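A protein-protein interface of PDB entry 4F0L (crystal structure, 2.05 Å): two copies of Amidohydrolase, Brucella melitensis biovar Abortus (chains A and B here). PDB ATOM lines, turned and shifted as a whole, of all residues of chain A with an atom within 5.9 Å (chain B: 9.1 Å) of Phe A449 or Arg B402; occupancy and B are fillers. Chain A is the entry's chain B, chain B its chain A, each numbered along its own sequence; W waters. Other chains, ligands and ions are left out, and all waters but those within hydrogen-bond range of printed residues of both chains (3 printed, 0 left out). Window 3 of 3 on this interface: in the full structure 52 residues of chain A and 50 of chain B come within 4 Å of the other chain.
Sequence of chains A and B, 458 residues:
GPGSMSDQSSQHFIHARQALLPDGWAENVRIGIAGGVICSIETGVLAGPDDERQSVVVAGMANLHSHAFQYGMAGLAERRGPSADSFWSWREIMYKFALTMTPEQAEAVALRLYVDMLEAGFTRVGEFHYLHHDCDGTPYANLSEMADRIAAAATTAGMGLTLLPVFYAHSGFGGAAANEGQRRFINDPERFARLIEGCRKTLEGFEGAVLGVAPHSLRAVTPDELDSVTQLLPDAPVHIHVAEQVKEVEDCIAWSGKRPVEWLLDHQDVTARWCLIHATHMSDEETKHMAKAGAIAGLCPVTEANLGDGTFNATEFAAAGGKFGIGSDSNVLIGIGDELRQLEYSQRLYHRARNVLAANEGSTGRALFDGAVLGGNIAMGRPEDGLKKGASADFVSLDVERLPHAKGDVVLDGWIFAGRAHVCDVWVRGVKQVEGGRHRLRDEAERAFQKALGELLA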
ATOM      1  N   TYR A  71       1.356  13.717  13.651  1.00  0.00           N
ATOM      2  CA  TYR A  71       1.929  12.880  12.586  1.00  0.00           C
ATOM      3  C   TYR A  71       1.666  11.405  12.881  1.00  0.00           C
ATOM      4  O   TYR A  71       1.526  10.602  11.973  1.00  0.00           O
ATOM      5  CB  TYR A  71       3.425  13.101  12.507  1.00  0.00           C
ATOM      6  CG  TYR A  71       4.214  12.342  11.440  1.00  0.00           C
ATOM      7  CD1 TYR A  71       4.115  12.665  10.084  1.00  0.00           C
ATOM      8  CD2 TYR A  71       5.136  11.358  11.818  1.00  0.00           C
ATOM      9  CE1 TYR A  71       4.861  11.987   9.124  1.00  0.00           C
ATOM     10  CE2 TYR A  71       5.903  10.696  10.886  1.00  0.00           C
ATOM     11  CZ  TYR A  71       5.754  11.001   9.525  1.00  0.00           C
ATOM     12  OH  TYR A  71       6.540  10.335   8.613  1.00  0.00           O
ATOM     13  N   GLY A  72       1.661  11.041  14.161  1.00  0.00           N
ATOM     14  CA  GLY A  72       1.370   9.661  14.543  1.00  0.00           C
ATOM     15  C   GLY A  72      -0.034   9.198  14.157  1.00  0.00           C
ATOM     16  O   GLY A  72      -0.254   8.018  13.941  1.00  0.00           O
ATOM     17  N   ALA A 108      10.492  10.358  19.168  1.00  0.00           N
ATOM     18  CA  ALA A 108      10.496   9.447  18.013  1.00  0.00           C
ATOM     19  C   ALA A 108       9.567   9.886  16.898  1.00  0.00           C
ATOM     20  O   ALA A 108       9.956   9.892  15.717  1.00  0.00           O
ATOM     21  CB  ALA A 108      10.141   8.032  18.443  1.00  0.00           C
ATOM     22  N   VAL A 109       8.346  10.255  17.253  1.00  0.00           N
ATOM     23  CA  VAL A 109       7.381  10.784  16.301  1.00  0.00           C
ATOM     24  C   VAL A 109       7.863  12.098  15.650  1.00  0.00           C
ATOM     25  O   VAL A 109       7.830  12.229  14.419  1.00  0.00           O
ATOM     26  CB  VAL A 109       6.014  10.986  16.949  1.00  0.00           C
ATOM     27  CG1 VAL A 109       5.056  11.686  15.997  1.00  0.00           C
ATOM     28  CG2 VAL A 109       5.455   9.629  17.408  1.00  0.00           C
ATOM     29  N   ARG A 112      10.746  11.472  13.128  1.00  0.00           N
ATOM     30  CA  ARG A 112      10.351  10.893  11.849  1.00  0.00           C
ATOM     31  C   ARG A 112       9.571  11.899  11.006  1.00  0.00           C
ATOM     32  O   ARG A 112       9.693  11.917   9.783  1.00  0.00           O
ATOM     33  CB  ARG A 112       9.546   9.611  12.053  1.00  0.00           C
ATOM     34  CG  ARG A 112       9.222   8.854  10.787  1.00  0.00           C
ATOM     35  CD  ARG A 112      10.502   8.372  10.092  1.00  0.00           C
ATOM     36  NE  ARG A 112      10.289   7.780   8.766  1.00  0.00           N
ATOM     37  CZ  ARG A 112      10.127   8.476   7.627  1.00  0.00           C
ATOM     38  NH1 ARG A 112      10.154   9.794   7.603  1.00  0.00           N
ATOM     39  NH2 ARG A 112       9.931   7.829   6.497  1.00  0.00           N
ATOM     40  N   ASP A 116      10.644  13.431   7.325  1.00  0.00           N
ATOM     41  CA  ASP A 116       9.674  13.525   6.232  1.00  0.00           C
ATOM     42  C   ASP A 116       9.622  14.988   5.668  1.00  0.00           C
ATOM     43  O   ASP A 116       9.664  15.221   4.452  1.00  0.00           O
ATOM     44  CB  ASP A 116       8.314  13.089   6.798  1.00  0.00           C
ATOM     45  CG  ASP A 116       7.490  12.308   5.828  1.00  0.00           C
ATOM     46  OD1 ASP A 116       7.504  12.727   4.647  1.00  0.00           O
ATOM     47  OD2 ASP A 116       6.778  11.328   6.260  1.00  0.00           O
ATOM     48  N   GLU A 444      16.601   4.538  10.389  1.00  0.00           N
ATOM     49  CA  GLU A 444      16.718   4.496  11.842  1.00  0.00           C
ATOM     50  C   GLU A 444      15.522   5.241  12.480  1.00  0.00           C
ATOM     51  O   GLU A 444      14.862   4.739  13.409  1.00  0.00           O
ATOM     52  CB  GLU A 444      18.039   5.157  12.295  1.00  0.00           C
ATOM     53  CG  GLU A 444      19.352   4.554  11.773  1.00  0.00           C
ATOM     54  CD  GLU A 444      19.830   5.051  10.397  1.00  0.00           C
ATOM     55  OE1 GLU A 444      19.057   5.665   9.636  1.00  0.00           O
ATOM     56  OE2 GLU A 444      21.010   4.767  10.045  1.00  0.00           O
ATOM     57  N   ALA A 445      15.218   6.419  11.957  1.00  0.00           N
ATOM     58  CA  ALA A 445      14.078   7.183  12.466  1.00  0.00           C
ATOM     59  C   ALA A 445      12.782   6.406  12.312  1.00  0.00           C
ATOM     60  O   ALA A 445      11.939   6.391  13.218  1.00  0.00           O
ATOM     61  CB  ALA A 445      13.976   8.533  11.783  1.00  0.00           C
ATOM     62  N   GLU A 446      12.625   5.747  11.166  1.00  0.00           N
ATOM     63  CA  GLU A 446      11.437   4.923  10.905  1.00  0.00           C
ATOM     64  C   GLU A 446      11.266   3.758  11.875  1.00  0.00           C
ATOM     65  O   GLU A 446      10.141   3.477  12.340  1.00  0.00           O
ATOM     66  CB  GLU A 446      11.477   4.404   9.469  1.00  0.00           C
ATOM     67  CG  GLU A 446      10.292   3.547   9.071  1.00  0.00           C
ATOM     68  CD  GLU A 446       8.969   4.300   9.073  1.00  0.00           C
ATOM     69  OE1 GLU A 446       8.911   5.531   9.308  1.00  0.00           O
ATOM     70  OE2 GLU A 446       7.956   3.625   8.843  1.00  0.00           O
ATOM     71  N   ARG A 447      12.351   3.040  12.148  1.00  0.00           N
ATOM     72  CA  ARG A 447      12.259   1.924  13.114  1.00  0.00           C
ATOM     73  C   ARG A 447      11.768   2.425  14.465  1.00  0.00           C
ATOM     74  O   ARG A 447      10.905   1.813  15.082  1.00  0.00           O
ATOM     75  CB  ARG A 447      13.584   1.187  13.275  1.00  0.00           C
ATOM     76  CG  ARG A 447      13.884   0.212  12.164  1.00  0.00           C
ATOM     77  CD  ARG A 447      15.154  -0.625  12.456  1.00  0.00           C
ATOM     78  NE  ARG A 447      16.393   0.167  12.293  1.00  0.00           N
ATOM     79  CZ  ARG A 447      17.049   0.355  11.137  1.00  0.00           C
ATOM     80  NH1 ARG A 447      18.150   1.104  11.100  1.00  0.00           N
ATOM     81  NH2 ARG A 447      16.642  -0.226  10.014  1.00  0.00           N
ATOM     82  N   ALA A 448      12.317   3.538  14.931  1.00  0.00           N
ATOM     83  CA  ALA A 448      11.895   4.083  16.215  1.00  0.00           C
ATOM     84  C   ALA A 448      10.423   4.570  16.154  1.00  0.00           C
ATOM     85  O   ALA A 448       9.653   4.375  17.097  1.00  0.00           O
ATOM     86  CB  ALA A 448      12.841   5.199  16.647  1.00  0.00           C
ATOM     87  N   PHE A 449      10.037   5.166  15.030  1.00  0.00           N
ATOM     88  CA  PHE A 449       8.661   5.608  14.835  1.00  0.00           C
ATOM     89  C   PHE A 449       7.668   4.440  14.875  1.00  0.00           C
ATOM     90  O   PHE A 449       6.645   4.542  15.542  1.00  0.00           O
ATOM     91  CB  PHE A 449       8.542   6.366  13.510  1.00  0.00           C
ATOM     92  CG  PHE A 449       7.146   6.774  13.153  1.00  0.00           C
ATOM     93  CD1 PHE A 449       6.438   7.679  13.929  1.00  0.00           C
ATOM     94  CD2 PHE A 449       6.534   6.253  12.017  1.00  0.00           C
ATOM     95  CE1 PHE A 449       5.141   8.051  13.605  1.00  0.00           C
ATOM     96  CE2 PHE A 449       5.237   6.630  11.691  1.00  0.00           C
ATOM     97  CZ  PHE A 449       4.542   7.533  12.489  1.00  0.00           C
ATOM     98  N   GLN A 450       7.968   3.341  14.181  1.00  0.00           N
ATOM     99  CA  GLN A 450       7.056   2.174  14.153  1.00  0.00           C
ATOM    100  C   GLN A 450       6.925   1.549  15.550  1.00  0.00           C
ATOM    101  O   GLN A 450       5.833   1.141  15.943  1.00  0.00           O
ATOM    102  CB  GLN A 450       7.497   1.108  13.139  1.00  0.00           C
ATOM    103  CG  GLN A 450       7.413   1.556  11.678  1.00  0.00           C
ATOM    104  CD  GLN A 450       5.990   1.873  11.257  1.00  0.00           C
ATOM    105  OE1 GLN A 450       5.051   1.317  11.796  1.00  0.00           O
ATOM    106  NE2 GLN A 450       5.833   2.791  10.326  1.00  0.00           N
ATOM    107  N   LYS A 451       8.014   1.551  16.321  1.00  0.00           N
ATOM    108  CA  LYS A 451       7.956   1.074  17.705  1.00  0.00           C
ATOM    109  C   LYS A 451       7.005   1.951  18.524  1.00  0.00           C
ATOM    110  O   LYS A 451       6.075   1.439  19.149  1.00  0.00           O
ATOM    111  CB  LYS A 451       9.358   1.048  18.309  1.00  0.00           C
ATOM    112  CG  LYS A 451       9.485   0.362  19.670  1.00  0.00           C
ATOM    113  CD  LYS A 451      10.956   0.357  20.118  1.00  0.00           C
ATOM    114  CE  LYS A 451      11.154   0.173  21.636  1.00  0.00           C
ATOM    115  NZ  LYS A 451      11.493  -1.216  22.080  1.00  0.00           N
ATOM    116  N   ALA A 452       7.174   3.271  18.459  1.00  0.00           N
ATOM    117  CA  ALA A 452       6.280   4.191  19.179  1.00  0.00           C
ATOM    118  C   ALA A 452       4.801   4.055  18.745  1.00  0.00           C
ATOM    119  O   ALA A 452       3.892   4.023  19.576  1.00  0.00           O
ATOM    120  CB  ALA A 452       6.754   5.640  19.055  1.00  0.00           C
ATOM    121  N   LEU A 453       4.563   3.923  17.451  1.00  0.00           N
ATOM    122  CA  LEU A 453       3.209   3.751  16.927  1.00  0.00           C
ATOM    123  C   LEU A 453       2.547   2.483  17.493  1.00  0.00           C
ATOM    124  O   LEU A 453       1.395   2.521  17.967  1.00  0.00           O
ATOM    125  CB  LEU A 453       3.256   3.736  15.381  1.00  0.00           C
ATOM    126  CG  LEU A 453       1.985   4.177  14.643  1.00  0.00           C
ATOM    127  CD1 LEU A 453       1.403   5.455  15.251  1.00  0.00           C
ATOM    128  CD2 LEU A 453       2.265   4.373  13.149  1.00  0.00           C
ATOM    129  N   GLY A 454       3.278   1.369  17.438  1.00  0.00           N
ATOM    130  CA  GLY A 454       2.821   0.125  18.001  1.00  0.00           C
ATOM    131  C   GLY A 454       2.410   0.282  19.448  1.00  0.00           C
ATOM    132  O   GLY A 454       1.367  -0.225  19.848  1.00  0.00           O
ATOM    133  N   LEU B 398       0.287  -3.324  -2.861  1.00  0.00           N
ATOM    134  CA  LEU B 398       0.706  -2.095  -2.234  1.00  0.00           C
ATOM    135  C   LEU B 398       1.910  -2.309  -1.342  1.00  0.00           C
ATOM    136  O   LEU B 398       1.954  -3.285  -0.610  1.00  0.00           O
ATOM    137  CB  LEU B 398      -0.450  -1.493  -1.431  1.00  0.00           C
ATOM    138  CG  LEU B 398      -1.689  -1.076  -2.281  1.00  0.00           C
ATOM    139  CD1 LEU B 398      -2.835  -0.662  -1.355  1.00  0.00           C
ATOM    140  CD2 LEU B 398      -1.359   0.032  -3.310  1.00  0.00           C
ATOM    141  N   ASP B 399       2.883  -1.395  -1.412  1.00  0.00           N
ATOM    142  CA  ASP B 399       4.040  -1.429  -0.505  1.00  0.00           C
ATOM    143  C   ASP B 399       3.573  -0.949   0.863  1.00  0.00           C
ATOM    144  O   ASP B 399       3.177   0.226   0.995  1.00  0.00           O
ATOM    145  CB  ASP B 399       5.166  -0.526  -1.040  1.00  0.00           C
ATOM    146  CG  ASP B 399       6.402  -0.530  -0.152  1.00  0.00           C
ATOM    147  OD1 ASP B 399       6.312  -0.689   1.067  1.00  0.00           O
ATOM    148  OD2 ASP B 399       7.504  -0.397  -0.704  1.00  0.00           O
ATOM    149  N   VAL B 400       3.580  -1.845   1.848  1.00  0.00           N
ATOM    150  CA  VAL B 400       3.122  -1.539   3.199  1.00  0.00           C
ATOM    151  C   VAL B 400       4.260  -1.591   4.215  1.00  0.00           C
ATOM    152  O   VAL B 400       4.035  -1.828   5.412  1.00  0.00           O
ATOM    153  CB  VAL B 400       1.992  -2.479   3.655  1.00  0.00           C
ATOM    154  CG1 VAL B 400       0.728  -2.180   2.842  1.00  0.00           C
ATOM    155  CG2 VAL B 400       2.422  -3.957   3.605  1.00  0.00           C
ATOM    156  N   GLU B 401       5.455  -1.277   3.750  1.00  0.00           N
ATOM    157  CA  GLU B 401       6.608  -1.219   4.629  1.00  0.00           C
ATOM    158  C   GLU B 401       6.378  -0.239   5.798  1.00  0.00           C
ATOM    159  O   GLU B 401       6.817  -0.523   6.888  1.00  0.00           O
ATOM    160  CB  GLU B 401       7.913  -0.877   3.865  1.00  0.00           C
ATOM    161  CG  GLU B 401       8.016   0.559   3.374  1.00  0.00           C
ATOM    162  CD  GLU B 401       9.285   0.869   2.591  1.00  0.00           C
ATOM    163  OE1 GLU B 401      10.387   0.641   3.148  1.00  0.00           O
ATOM    164  OE2 GLU B 401       9.165   1.350   1.424  1.00  0.00           O
ATOM    165  N   ARG B 402       5.672   0.872   5.575  1.00  0.00           N
ATOM    166  CA  ARG B 402       5.347   1.822   6.667  1.00  0.00           C
ATOM    167  C   ARG B 402       4.044   1.485   7.438  1.00  0.00           C
ATOM    168  O   ARG B 402       3.698   2.181   8.389  1.00  0.00           O
ATOM    169  CB  ARG B 402       5.321   3.261   6.148  1.00  0.00           C
ATOM    170  CG  ARG B 402       6.630   3.690   5.432  1.00  0.00           C
ATOM    171  CD  ARG B 402       6.803   5.203   5.405  1.00  0.00           C
ATOM    172  NE  ARG B 402       6.921   5.758   6.757  1.00  0.00           N
ATOM    173  CZ  ARG B 402       6.695   7.026   7.102  1.00  0.00           C
ATOM    174  NH1 ARG B 402       6.310   7.936   6.194  1.00  0.00           N
ATOM    175  NH2 ARG B 402       6.825   7.385   8.381  1.00  0.00           N
ATOM    176  N   LEU B 403       3.341   0.428   7.031  1.00  0.00           N
ATOM    177  CA  LEU B 403       2.079  -0.018   7.676  1.00  0.00           C
ATOM    178  C   LEU B 403       2.115  -1.535   7.809  1.00  0.00           C
ATOM    179  O   LEU B 403       1.198  -2.223   7.341  1.00  0.00           O
ATOM    180  CB  LEU B 403       0.921   0.379   6.772  1.00  0.00           C
ATOM    181  CG  LEU B 403       0.621   1.877   6.577  1.00  0.00           C
ATOM    182  CD1 LEU B 403      -0.358   2.141   5.462  1.00  0.00           C
ATOM    183  CD2 LEU B 403       0.069   2.463   7.872  1.00  0.00           C
ATOM    184  N   PRO B 404       3.178  -2.075   8.423  1.00  0.00           N
ATOM    185  CA  PRO B 404       3.574  -3.477   8.192  1.00  0.00           C
ATOM    186  C   PRO B 404       2.562  -4.582   8.562  1.00  0.00           C
ATOM    187  O   PRO B 404       2.562  -5.639   7.924  1.00  0.00           O
ATOM    188  CB  PRO B 404       4.870  -3.613   9.018  1.00  0.00           C
ATOM    189  CG  PRO B 404       4.811  -2.493   9.999  1.00  0.00           C
ATOM    190  CD  PRO B 404       4.193  -1.375   9.224  1.00  0.00           C
ATOM    191  N   HIS B 405       1.741  -4.370   9.584  1.00  0.00           N
ATOM    192  CA  HIS B 405       0.645  -5.325   9.883  1.00  0.00           C
ATOM    193  C   HIS B 405      -0.725  -4.691   9.926  1.00  0.00           C
ATOM    194  O   HIS B 405      -1.677  -5.318  10.416  1.00  0.00           O
ATOM    195  CB  HIS B 405       0.961  -6.053  11.173  1.00  0.00           C
ATOM    196  CG  HIS B 405       2.269  -6.788  11.126  1.00  0.00           C
ATOM    197  ND1 HIS B 405       2.416  -7.986  10.470  1.00  0.00           N
ATOM    198  CD2 HIS B 405       3.518  -6.463  11.654  1.00  0.00           C
ATOM    199  CE1 HIS B 405       3.705  -8.381  10.592  1.00  0.00           C
ATOM    200  NE2 HIS B 405       4.369  -7.450  11.317  1.00  0.00           N
ATOM    201  N   ALA B 406      -0.837  -3.478   9.376  1.00  0.00           N
ATOM    202  CA  ALA B 406      -2.089  -2.735   9.377  1.00  0.00           C
ATOM    203  C   ALA B 406      -3.184  -3.453   8.607  1.00  0.00           C
ATOM    204  O   ALA B 406      -2.953  -4.078   7.564  1.00  0.00           O
ATOM    205  CB  ALA B 406      -1.879  -1.339   8.834  1.00  0.00           C
ATOM    206  N   VAL B 410      -7.162   0.458   6.776  1.00  0.00           N
ATOM    207  CA  VAL B 410      -6.117   1.352   7.267  1.00  0.00           C
ATOM    208  C   VAL B 410      -5.067   1.526   6.175  1.00  0.00           C
ATOM    209  O   VAL B 410      -4.562   2.656   5.944  1.00  0.00           O
ATOM    210  CB  VAL B 410      -5.496   0.841   8.584  1.00  0.00           C
ATOM    211  CG1 VAL B 410      -4.221   1.646   8.915  1.00  0.00           C
ATOM    212  CG2 VAL B 410      -6.515   0.910   9.723  1.00  0.00           C
ATOM    213  N   VAL B 411      -4.788   0.453   5.435  1.00  0.00           N
ATOM    214  CA  VAL B 411      -3.827   0.545   4.335  1.00  0.00           C
ATOM    215  C   VAL B 411      -4.350   1.477   3.238  1.00  0.00           C
ATOM    216  O   VAL B 411      -3.603   2.331   2.745  1.00  0.00           O
ATOM    217  CB  VAL B 411      -3.402  -0.835   3.762  1.00  0.00           C
ATOM    218  CG1 VAL B 411      -2.490  -0.677   2.547  1.00  0.00           C
ATOM    219  CG2 VAL B 411      -2.609  -1.635   4.791  1.00  0.00           C
ATOM    220  N   GLY B 414      -4.179   5.075   4.304  1.00  0.00           N
ATOM    221  CA  GLY B 414      -2.801   5.504   4.372  1.00  0.00           C
ATOM    222  C   GLY B 414      -2.283   5.842   3.001  1.00  0.00           C
ATOM    223  O   GLY B 414      -1.556   6.827   2.779  1.00  0.00           O
ATOM    224  N   ALA B 418      -2.624   9.804   3.443  1.00  0.00           N
ATOM    225  CA  ALA B 418      -1.462  10.125   4.290  1.00  0.00           C
ATOM    226  C   ALA B 418      -0.114   9.855   3.616  1.00  0.00           C
ATOM    227  O   ALA B 418       0.896  10.083   4.245  1.00  0.00           O
ATOM    228  CB  ALA B 418      -1.563   9.418   5.651  1.00  0.00           C
ATOM    229  N   GLY B 419      -0.088   9.384   2.365  1.00  0.00           N
ATOM    230  CA  GLY B 419       1.200   9.100   1.653  1.00  0.00           C
ATOM    231  C   GLY B 419       2.040   7.974   2.274  1.00  0.00           C
ATOM    232  O   GLY B 419       3.267   7.900   2.072  1.00  0.00           O
ATOM    233  N   ARG B 420       1.382   7.079   3.013  1.00  0.00           N
ATOM    234  CA  ARG B 420       2.069   6.054   3.804  1.00  0.00           C
ATOM    235  C   ARG B 420       2.186   4.662   3.132  1.00  0.00           C
ATOM    236  O   ARG B 420       2.716   3.723   3.711  1.00  0.00           O
ATOM    237  CB  ARG B 420       1.325   5.894   5.138  1.00  0.00           C
ATOM    238  CG  ARG B 420       1.513   7.069   6.107  1.00  0.00           C
ATOM    239  CD  ARG B 420       2.912   7.192   6.725  1.00  0.00           C
ATOM    240  NE  ARG B 420       2.938   8.464   7.486  1.00  0.00           N
ATOM    241  CZ  ARG B 420       2.572   8.605   8.746  1.00  0.00           C
ATOM    242  NH1 ARG B 420       2.277   7.547   9.484  1.00  0.00           N
ATOM    243  NH2 ARG B 420       2.559   9.815   9.293  1.00  0.00           N
ATOM    244  N   ALA B 421       1.625   4.526   1.945  1.00  0.00           N
ATOM    245  CA  ALA B 421       1.754   3.303   1.162  1.00  0.00           C
ATOM    246  C   ALA B 421       1.795   3.751  -0.287  1.00  0.00           C
ATOM    247  O   ALA B 421       1.370   4.880  -0.601  1.00  0.00           O
ATOM    248  CB  ALA B 421       0.579   2.396   1.428  1.00  0.00           C
ATOM    249  N   HIS B 422       2.342   2.903  -1.154  1.00  0.00           N
ATOM    250  CA  HIS B 422       2.470   3.190  -2.584  1.00  0.00           C
ATOM    251  C   HIS B 422       2.310   1.917  -3.394  1.00  0.00           C
ATOM    252  O   HIS B 422       2.454   0.818  -2.860  1.00  0.00           O
ATOM    253  CB  HIS B 422       3.854   3.823  -2.860  1.00  0.00           C
ATOM    254  CG  HIS B 422       4.171   4.978  -1.959  1.00  0.00           C
ATOM    255  ND1 HIS B 422       3.907   6.266  -2.291  1.00  0.00           N
ATOM    256  CD2 HIS B 422       4.730   5.008  -0.682  1.00  0.00           C
ATOM    257  CE1 HIS B 422       4.284   7.080  -1.293  1.00  0.00           C
ATOM    258  NE2 HIS B 422       4.788   6.308  -0.296  1.00  0.00           N
HETATM  259  O   HOH W   1       0.011   7.302  11.410  1.00  0.00           O
HETATM  260  O   HOH W   2       8.620   1.165   8.156  1.00  0.00           O
HETATM  261  O   HOH W   3       3.912  10.098   5.156  1.00  0.00           O
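NH2 of Arg B402 is in hydrogen-bond range of OH of Tyr A71.
The guanidinium group (NH2) of Arg B420 lies within hydrogen-bond range of the backbone carbonyl oxygen (O) of Tyr A71.
NH1 of Arg B402 lies within salt-bridge range of OD2 of Asp A116, at 3.4 Å.
NH2 of Arg B402 is in salt-bridge range of OE1 of Glu A446 (2.9 Å).
The backbone carbonyl oxygen (O) of Arg B402 sits at hydrogen-bond distance from the side-chain amide nitrogen (NE2) of Gln A450, 2.9 Å away.
The side-chain hydroxyl of Tyr A71 is in hydrogen-bond range of the side-chain carboxylate of Asp A116 (2.6 Å).
NE of Arg A112 lies within salt-bridge range of OE1 of Glu A446, 2.7 Å away.
The side-chain carboxylate of Glu A446 is in hydrogen-bond range of the side-chain amide nitrogen of Gln A450 (2.7 Å).
The guanidinium group (NH1) of Arg A112 is in salt-bridge range of the side-chain carboxylate (OD2) of Asp A116, 3.9 Å away.
The backbone carbonyl oxygen of Gly B414 sits at hydrogen-bond distance from the backbone NH of Arg B420 (3.0 Å).
Arg A112 touches Arg B402.
NH2 of Arg B402 touches CE2 of Phe A449 (3.7 Å).
Arg B420 touches Phe A449 (NH1 to CZ, 3.8 Å).
OE1 of Gln A450 touches CD of Pro B404, 3.8 Å away.
Of chain B, only Arg B402 and Arg B420 come within 4 Å of Phe A449.
Of chain A, only Tyr A71, Arg A112, Asp A116, Glu A446, Phe A449 and Gln A450 come within 4 Å of Arg B402.
No residue of chain B comes within 4 Å of Ala A448.
Gln A450 touches just these residues of chain B: Arg B402 (2.9 Å) and Pro B404 (3.8 Å).
Of the printed residues of chain A, Pro B404 touches Gln A450 (3.8 Å).
Printed residues of chain B within 4 Å of Glu A446: Arg B402 (2.9 Å).
Printed residues of chain A within 4 Å of Arg B420: Tyr A71 and Phe A449.
Printed residues of chain B within 4 Å of Asp A116: Arg B402 (3.4 Å).
Printed residues of chain B within 4 Å of Arg A112: Arg B402 (3.4 Å).
Ala B421 touches none of the printed residues of chain A.
The nearest residue of chain B that does not touch Phe A449 is Leu B403 (7.7 Å).
The nearest residue of chain A that does not touch Arg B402 is Leu A453 (5.4 Å).
The nearest printed residue of chain B that does not touch Tyr A71 is Ala B418 (6.6 Å).
Of the 17 printed residues of chain A, 6 touch a printed residue of chain B.
Hydrophobic or aromatic side chains of chain A that line the printed part of chain B: Tyr A71 and Phe A449.
Among the printed residues, Asp or Glu carboxylates within 4 Å of a Lys or Arg side-chain nitrogen of the other chain: Asp A116 with Arg B402 (3.4 Å) and Glu A446 with Arg B402 (2.9 Å).
No position is printed for both chains.
Of the 9 pairs that touch across the chains among the printed residues, none has its exchanged pair printed and touching as well.
Water W2 bridges OE2 of Glu A446 (2.6 Å) and O of Glu B401 (2.8 Å).
Water W1 lies within hydrogen-bond range of the backbone carbonyl oxygen (O) of Gly A72 (2.6 Å) and the guanidinium group (NH1) of Arg B420 (3.0 Å).
Water W3 lies within hydrogen-bond range of NE of Arg B420, O of Ala B418, OD2 of Asp A116 and NH1 of Arg B402.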
